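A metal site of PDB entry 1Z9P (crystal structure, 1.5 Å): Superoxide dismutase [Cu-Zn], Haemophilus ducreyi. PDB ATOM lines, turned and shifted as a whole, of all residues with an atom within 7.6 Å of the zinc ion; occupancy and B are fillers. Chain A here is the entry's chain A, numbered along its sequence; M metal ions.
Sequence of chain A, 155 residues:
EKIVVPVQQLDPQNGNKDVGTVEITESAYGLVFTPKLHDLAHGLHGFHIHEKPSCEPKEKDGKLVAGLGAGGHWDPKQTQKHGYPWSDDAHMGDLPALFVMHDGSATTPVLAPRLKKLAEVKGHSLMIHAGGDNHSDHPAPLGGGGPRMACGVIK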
ATOM      1  N   PHE A  47      11.760  10.142  -0.907  1.00  0.00           N
ATOM      2  CA  PHE A  47      11.588  11.337  -1.700  1.00  0.00           C
ATOM      3  C   PHE A  47      13.009  11.805  -2.057  1.00  0.00           C
ATOM      4  O   PHE A  47      13.794  12.181  -1.202  1.00  0.00           O
ATOM      5  CB  PHE A  47      10.836  12.316  -0.846  1.00  0.00           C
ATOM      6  CG  PHE A  47      10.465  13.654  -1.505  1.00  0.00           C
ATOM      7  CD1 PHE A  47       9.921  13.724  -2.788  1.00  0.00           C
ATOM      8  CD2 PHE A  47      10.480  14.789  -0.762  1.00  0.00           C
ATOM      9  CE1 PHE A  47       9.510  14.970  -3.307  1.00  0.00           C
ATOM     10  CE2 PHE A  47      10.077  16.022  -1.255  1.00  0.00           C
ATOM     11  CZ  PHE A  47       9.575  16.091  -2.544  1.00  0.00           C
ATOM     12  N   HIS A  48      13.329  11.679  -3.341  1.00  0.00           N
ATOM     13  CA  HIS A  48      14.687  11.987  -3.803  1.00  0.00           C
ATOM     14  C   HIS A  48      14.722  12.697  -5.148  1.00  0.00           C
ATOM     15  O   HIS A  48      13.844  12.528  -5.972  1.00  0.00           O
ATOM     16  CB  HIS A  48      15.617  10.761  -3.886  1.00  0.00           C
ATOM     17  CG  HIS A  48      15.259   9.642  -2.955  1.00  0.00           C
ATOM     18  ND1 HIS A  48      14.683   8.475  -3.402  1.00  0.00           N
ATOM     19  CD2 HIS A  48      15.427   9.522  -1.613  1.00  0.00           C
ATOM     20  CE1 HIS A  48      14.479   7.679  -2.354  1.00  0.00           C
ATOM     21  NE2 HIS A  48      14.920   8.279  -1.271  1.00  0.00           N
ATOM     22  N   ILE A  49      15.802  13.440  -5.344  1.00  0.00           N
ATOM     23  CA  ILE A  49      16.136  13.972  -6.674  1.00  0.00           C
ATOM     24  C   ILE A  49      17.005  12.942  -7.363  1.00  0.00           C
ATOM     25  O   ILE A  49      17.998  12.468  -6.788  1.00  0.00           O
ATOM     26  CB  ILE A  49      16.848  15.306  -6.570  1.00  0.00           C
ATOM     27  CG1 ILE A  49      15.972  16.299  -5.797  1.00  0.00           C
ATOM     28  CG2 ILE A  49      17.127  15.839  -7.959  1.00  0.00           C
ATOM     29  CD1 ILE A  49      16.627  17.661  -5.634  1.00  0.00           C
ATOM     30  N   HIS A  50      16.555  12.530  -8.548  1.00  0.00           N
ATOM     31  CA  HIS A  50      17.293  11.553  -9.362  1.00  0.00           C
ATOM     32  C   HIS A  50      17.989  12.314 -10.481  1.00  0.00           C
ATOM     33  O   HIS A  50      17.674  13.457 -10.799  1.00  0.00           O
ATOM     34  CB  HIS A  50      16.373  10.450  -9.920  1.00  0.00           C
ATOM     35  CG  HIS A  50      15.951   9.432  -8.901  1.00  0.00           C
ATOM     36  ND1 HIS A  50      16.123   8.078  -9.081  1.00  0.00           N
ATOM     37  CD2 HIS A  50      15.365   9.581  -7.696  1.00  0.00           C
ATOM     38  CE1 HIS A  50      15.629   7.436  -8.029  1.00  0.00           C
ATOM     39  NE2 HIS A  50      15.203   8.320  -7.162  1.00  0.00           N
ATOM     40  N   GLY A  72      19.670   6.925 -11.309  1.00  0.00           N
ATOM     41  CA  GLY A  72      19.872   6.805  -9.901  1.00  0.00           C
ATOM     42  C   GLY A  72      19.733   8.123  -9.200  1.00  0.00           C
ATOM     43  O   GLY A  72      19.350   9.134  -9.801  1.00  0.00           O
ATOM     44  N   HIS A  73      20.043   8.109  -7.929  1.00  0.00           N
ATOM     45  CA  HIS A  73      20.008   9.319  -7.110  1.00  0.00           C
ATOM     46  C   HIS A  73      21.034  10.333  -7.608  1.00  0.00           C
ATOM     47  O   HIS A  73      22.148   9.996  -8.042  1.00  0.00           O
ATOM     48  CB  HIS A  73      20.227   8.990  -5.666  1.00  0.00           C
ATOM     49  CG  HIS A  73      19.122   8.173  -5.070  1.00  0.00           C
ATOM     50  ND1 HIS A  73      18.948   8.029  -3.717  1.00  0.00           N
ATOM     51  CD2 HIS A  73      18.103   7.484  -5.642  1.00  0.00           C
ATOM     52  CE1 HIS A  73      17.915   7.250  -3.472  1.00  0.00           C
ATOM     53  NE2 HIS A  73      17.379   6.910  -4.626  1.00  0.00           N
ATOM     54  N   TRP A  74      20.648  11.590  -7.558  1.00  0.00           N
ATOM     55  CA  TRP A  74      21.470  12.654  -8.052  1.00  0.00           C
ATOM     56  C   TRP A  74      22.662  12.751  -7.108  1.00  0.00           C
ATOM     57  O   TRP A  74      22.520  12.931  -5.926  1.00  0.00           O
ATOM     58  CB  TRP A  74      20.696  13.966  -8.074  1.00  0.00           C
ATOM     59  CG  TRP A  74      21.474  15.179  -8.493  1.00  0.00           C
ATOM     60  CD1 TRP A  74      22.403  15.326  -9.542  1.00  0.00           C
ATOM     61  CD2 TRP A  74      21.406  16.448  -7.885  1.00  0.00           C
ATOM     62  NE1 TRP A  74      22.859  16.609  -9.586  1.00  0.00           N
ATOM     63  CE2 TRP A  74      22.276  17.334  -8.582  1.00  0.00           C
ATOM     64  CE3 TRP A  74      20.664  16.965  -6.801  1.00  0.00           C
ATOM     65  CZ2 TRP A  74      22.410  18.655  -8.221  1.00  0.00           C
ATOM     66  CZ3 TRP A  74      20.809  18.283  -6.449  1.00  0.00           C
ATOM     67  CH2 TRP A  74      21.673  19.122  -7.163  1.00  0.00           C
ATOM     68  N   ASP A  75      23.877  12.632  -7.652  1.00  0.00           N
ATOM     69  CA  ASP A  75      25.064  12.439  -6.828  1.00  0.00           C
ATOM     70  C   ASP A  75      26.243  13.128  -7.502  1.00  0.00           C
ATOM     71  O   ASP A  75      27.210  12.447  -7.920  1.00  0.00           O
ATOM     72  CB  ASP A  75      25.308  10.938  -6.648  1.00  0.00           C
ATOM     73  CG  ASP A  75      26.456  10.617  -5.662  1.00  0.00           C
ATOM     74  OD1 ASP A  75      26.762  11.431  -4.755  1.00  0.00           O
ATOM     75  OD2 ASP A  75      27.032   9.502  -5.672  1.00  0.00           O
ATOM     76  N   THR A  79      29.408  10.584  -3.924  1.00  0.00           N
ATOM     77  CA  THR A  79      29.569   9.888  -2.645  1.00  0.00           C
ATOM     78  C   THR A  79      29.307   8.395  -2.745  1.00  0.00           C
ATOM     79  O   THR A  79      29.773   7.634  -1.887  1.00  0.00           O
ATOM     80  CB  THR A  79      28.612  10.438  -1.543  1.00  0.00           C
ATOM     81  OG1 THR A  79      27.229  10.209  -1.899  1.00  0.00           O
ATOM     82  CG2 THR A  79      28.746  11.943  -1.366  1.00  0.00           C
ATOM     83  N   LYS A  81      26.779   6.890  -1.861  1.00  0.00           N
ATOM     84  CA  LYS A  81      26.176   6.483  -0.620  1.00  0.00           C
ATOM     85  C   LYS A  81      24.829   7.184  -0.451  1.00  0.00           C
ATOM     86  O   LYS A  81      24.780   8.421  -0.548  1.00  0.00           O
ATOM     87  CB  LYS A  81      27.092   6.819   0.567  1.00  0.00           C
ATOM     88  CG  LYS A  81      26.493   6.676   1.946  1.00  0.00           C
ATOM     89  CD  LYS A  81      27.489   7.005   3.039  1.00  0.00           C
ATOM     90  CE  LYS A  81      26.922   6.639   4.407  1.00  0.00           C
ATOM     91  NZ  LYS A  81      27.587   7.398   5.487  1.00  0.00           N
ATOM     92  N   HIS A  82      23.769   6.404  -0.241  1.00  0.00           N
ATOM     93  CA  HIS A  82      22.487   6.978   0.154  1.00  0.00           C
ATOM     94  C   HIS A  82      22.542   7.277   1.636  1.00  0.00           C
ATOM     95  O   HIS A  82      23.046   6.469   2.440  1.00  0.00           O
ATOM     96  CB  HIS A  82      21.353   5.993  -0.117  1.00  0.00           C
ATOM     97  CG  HIS A  82      20.010   6.540   0.195  1.00  0.00           C
ATOM     98  ND1 HIS A  82      19.434   7.535  -0.580  1.00  0.00           N
ATOM     99  CD2 HIS A  82      19.130   6.298   1.205  1.00  0.00           C
ATOM    100  CE1 HIS A  82      18.263   7.856  -0.062  1.00  0.00           C
ATOM    101  NE2 HIS A  82      18.061   7.145   1.023  1.00  0.00           N
ATOM    102  N   GLY A  83      22.005   8.435   2.047  1.00  0.00           N
ATOM    103  CA  GLY A  83      22.115   8.811   3.438  1.00  0.00           C
ATOM    104  C   GLY A  83      21.139   9.864   3.875  1.00  0.00           C
ATOM    105  O   GLY A  83      20.077   9.984   3.246  1.00  0.00           O
ATOM    106  N   TYR A  84      21.475  10.627   4.917  1.00  0.00           N
ATOM    107  CA  TYR A  84      20.598  11.604   5.505  1.00  0.00           C
ATOM    108  C   TYR A  84      20.628  12.932   4.757  1.00  0.00           C
ATOM    109  O   TYR A  84      21.653  13.298   4.166  1.00  0.00           O
ATOM    110  CB  TYR A  84      20.968  11.871   6.969  1.00  0.00           C
ATOM    111  CG  TYR A  84      20.785  10.696   7.875  1.00  0.00           C
ATOM    112  CD1 TYR A  84      21.825   9.846   8.150  1.00  0.00           C
ATOM    113  CD2 TYR A  84      19.572  10.410   8.398  1.00  0.00           C
ATOM    114  CE1 TYR A  84      21.655   8.744   8.991  1.00  0.00           C
ATOM    115  CE2 TYR A  84      19.365   9.297   9.207  1.00  0.00           C
ATOM    116  CZ  TYR A  84      20.422   8.483   9.494  1.00  0.00           C
ATOM    117  OH  TYR A  84      20.225   7.374  10.314  1.00  0.00           O
ATOM    118  N   ALA A  90      26.244  11.770   1.824  1.00  0.00           N
ATOM    119  CA  ALA A  90      25.086  11.221   1.171  1.00  0.00           C
ATOM    120  C   ALA A  90      24.833  11.882  -0.180  1.00  0.00           C
ATOM    121  O   ALA A  90      25.295  13.029  -0.424  1.00  0.00           O
ATOM    122  CB  ALA A  90      23.891  11.420   2.104  1.00  0.00           C
ATOM    123  N   HIS A  91      24.042  11.227  -1.053  1.00  0.00           N
ATOM    124  CA  HIS A  91      23.711  11.780  -2.379  1.00  0.00           C
ATOM    125  C   HIS A  91      23.122  13.170  -2.162  1.00  0.00           C
ATOM    126  O   HIS A  91      22.311  13.379  -1.253  1.00  0.00           O
ATOM    127  CB  HIS A  91      22.632  10.989  -3.105  1.00  0.00           C
ATOM    128  CG  HIS A  91      22.946   9.540  -3.261  1.00  0.00           C
ATOM    129  ND1 HIS A  91      22.057   8.548  -2.934  1.00  0.00           N
ATOM    130  CD2 HIS A  91      24.049   8.921  -3.756  1.00  0.00           C
ATOM    131  CE1 HIS A  91      22.601   7.363  -3.199  1.00  0.00           C
ATOM    132  NE2 HIS A  91      23.807   7.569  -3.709  1.00  0.00           N
ATOM    133  N   MET A  92      23.479  14.128  -3.001  1.00  0.00           N
ATOM    134  CA  MET A  92      22.897  15.470  -2.937  1.00  0.00           C
ATOM    135  C   MET A  92      21.380  15.415  -3.130  1.00  0.00           C
ATOM    136  O   MET A  92      20.665  16.280  -2.606  1.00  0.00           O
ATOM    137  CB  MET A  92      23.450  16.388  -4.016  1.00  0.00           C
ATOM    138  CG  MET A  92      23.380  17.826  -3.672  1.00  0.00           C
ATOM    139  SD  MET A  92      24.475  18.336  -2.340  1.00  0.00           S
ATOM    140  CE  MET A  92      24.561  20.042  -2.821  1.00  0.00           C
ATOM    141  N   GLY A  93      20.901  14.393  -3.823  1.00  0.00           N
ATOM    142  CA  GLY A  93      19.440  14.239  -4.032  1.00  0.00           C
ATOM    143  C   GLY A  93      18.649  13.701  -2.866  1.00  0.00           C
ATOM    144  O   GLY A  93      17.423  13.523  -2.999  1.00  0.00           O
ATOM    145  N   ASP A  94      19.290  13.410  -1.756  1.00  0.00           N
ATOM    146  CA  ASP A  94      18.570  12.753  -0.641  1.00  0.00           C
ATOM    147  C   ASP A  94      17.778  13.778   0.195  1.00  0.00           C
ATOM    148  O   ASP A  94      18.335  14.559   0.918  1.00  0.00           O
ATOM    149  CB  ASP A  94      19.515  11.977   0.275  1.00  0.00           C
ATOM    150  CG  ASP A  94      20.110  10.801  -0.429  1.00  0.00           C
ATOM    151  OD1 ASP A  94      19.610  10.446  -1.533  1.00  0.00           O
ATOM    152  OD2 ASP A  94      21.108  10.186   0.063  1.00  0.00           O
ATOM    153  N   LEU A  95      16.442  13.698   0.113  1.00  0.00           N
ATOM    154  CA  LEU A  95      15.547  14.641   0.794  1.00  0.00           C
ATOM    155  C   LEU A  95      14.854  13.949   1.966  1.00  0.00           C
ATOM    156  O   LEU A  95      14.858  12.704   2.008  1.00  0.00           O
ATOM    157  CB  LEU A  95      14.456  15.195  -0.153  1.00  0.00           C
ATOM    158  CG  LEU A  95      14.926  15.567  -1.565  1.00  0.00           C
ATOM    159  CD1 LEU A  95      13.712  15.915  -2.493  1.00  0.00           C
ATOM    160  CD2 LEU A  95      15.875  16.730  -1.549  1.00  0.00           C
ATOM    161  N   ARG A 114      21.252  20.986   2.364  1.00  0.00           N
ATOM    162  CA  ARG A 114      22.460  21.011   1.510  1.00  0.00           C
ATOM    163  C   ARG A 114      22.219  21.629   0.153  1.00  0.00           C
ATOM    164  O   ARG A 114      23.177  21.855  -0.612  1.00  0.00           O
ATOM    165  CB  ARG A 114      23.052  19.633   1.363  1.00  0.00           C
ATOM    166  CG  ARG A 114      23.577  19.138   2.630  1.00  0.00           C
ATOM    167  CD  ARG A 114      24.239  17.761   2.480  1.00  0.00           C
ATOM    168  NE  ARG A 114      23.253  16.687   2.285  1.00  0.00           N
ATOM    169  CZ  ARG A 114      23.364  15.680   1.411  1.00  0.00           C
ATOM    170  NH1 ARG A 114      24.354  15.618   0.560  1.00  0.00           N
ATOM    171  NH2 ARG A 114      22.424  14.748   1.397  1.00  0.00           N
ATOM    172  N   ASP A 133      12.050   5.545   3.763  1.00  0.00           N
ATOM    173  CA  ASP A 133      13.450   5.860   3.588  1.00  0.00           C
ATOM    174  C   ASP A 133      14.145   5.827   4.950  1.00  0.00           C
ATOM    175  O   ASP A 133      13.944   6.704   5.781  1.00  0.00           O
ATOM    176  CB  ASP A 133      13.609   7.268   2.924  1.00  0.00           C
ATOM    177  CG  ASP A 133      14.996   7.531   2.385  1.00  0.00           C
ATOM    178  OD1 ASP A 133      15.963   6.794   2.722  1.00  0.00           O
ATOM    179  OD2 ASP A 133      15.215   8.497   1.612  1.00  0.00           O
ATOM    180  N   HIS A 135      17.373   6.198   5.087  1.00  0.00           N
ATOM    181  CA  HIS A 135      18.575   6.975   4.862  1.00  0.00           C
ATOM    182  C   HIS A 135      19.832   6.166   5.054  1.00  0.00           C
ATOM    183  O   HIS A 135      20.846   6.631   5.579  1.00  0.00           O
ATOM    184  CB  HIS A 135      18.601   8.204   5.766  1.00  0.00           C
ATOM    185  CG  HIS A 135      17.464   9.137   5.528  1.00  0.00           C
ATOM    186  ND1 HIS A 135      17.330   9.871   4.367  1.00  0.00           N
ATOM    187  CD2 HIS A 135      16.383   9.417   6.279  1.00  0.00           C
ATOM    188  CE1 HIS A 135      16.205  10.562   4.427  1.00  0.00           C
ATOM    189  NE2 HIS A 135      15.615  10.303   5.570  1.00  0.00           N
ATOM    190  N   ASP A 137      21.831   2.559   2.873  1.00  0.00           N
ATOM    191  CA  ASP A 137      21.762   1.420   1.956  1.00  0.00           C
ATOM    192  C   ASP A 137      21.681   0.094   2.709  1.00  0.00           C
ATOM    193  O   ASP A 137      21.570  -0.963   2.089  1.00  0.00           O
ATOM    194  CB  ASP A 137      22.957   1.395   1.043  1.00  0.00           C
ATOM    195  CG  ASP A 137      23.001   2.571   0.112  1.00  0.00           C
ATOM    196  OD1 ASP A 137      22.164   2.637  -0.834  1.00  0.00           O
ATOM    197  OD2 ASP A 137      23.851   3.458   0.256  1.00  0.00           O
ATOM    198  N   LEU A 142      19.203   2.188  -1.201  1.00  0.00           N
ATOM    199  CA  LEU A 142      18.526   3.455  -1.471  1.00  0.00           C
ATOM    200  C   LEU A 142      17.392   3.662  -0.450  1.00  0.00           C
ATOM    201  O   LEU A 142      16.302   4.171  -0.772  1.00  0.00           O
ATOM    202  CB  LEU A 142      18.059   3.525  -2.925  1.00  0.00           C
ATOM    203  CG  LEU A 142      19.202   3.366  -3.960  1.00  0.00           C
ATOM    204  CD1 LEU A 142      18.619   3.121  -5.307  1.00  0.00           C
ATOM    205  CD2 LEU A 142      20.179   4.561  -4.046  1.00  0.00           C
ATOM    206  N   GLY A 143      17.663   3.279   0.785  1.00  0.00           N
ATOM    207  CA  GLY A 143      16.763   3.493   1.882  1.00  0.00           C
ATOM    208  C   GLY A 143      15.508   2.674   1.946  1.00  0.00           C
ATOM    209  O   GLY A 143      14.678   2.888   2.840  1.00  0.00           O
HETATM  210 ZN    ZN M   1      20.140   8.646  -2.186  1.00  0.00          ZN
HETATM  211 CU    CU M   2      14.534   7.907  -5.337  1.00  0.00          CU
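The backbone NH (N) of His 91 sits at hydrogen-bond distance from the backbone carbonyl oxygen (O) of Lys 81 (2.9 Å). A ring nitrogen (NE2) of His 82 lies within hydrogen-bond range of the side-chain carboxylate (OD1) of Asp 133 (2.7 Å). The backbone NH (N) of His 91 lies within hydrogen-bond range of the side-chain hydroxyl (OG1) of Thr 79 (3.5 Å). The side-chain carboxylate (OD2) of Asp 137 is in hydrogen-bond range of the backbone NH (N) of His 82, at 3.0 Å. The backbone NH of Gly 83 lies within hydrogen-bond range of the side-chain carboxylate of Asp 94 (2.8 Å). ND1 of His 48 lies close to NE2 of His 73 (3.3 Å). O of His 91 lies within hydrogen-bond range of NH2 of Arg 114 (3.0 Å).
The side-chain carboxylate (OD1) of Asp 94 is bound to the zinc ion (2.0 Å). ND1 of His 73 is bound to the zinc ion, at 2.0 Å. ND1 of His 91 binds the zinc ion. The zinc ion is bound by ND1 of His 82, 2.1 Å away.
Within 4 Å of the zinc ion: His 73, His 82, His 91 and Asp 94. The nearest printed residue that does not touch the zinc ion is Leu 142 (4.5 Å).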
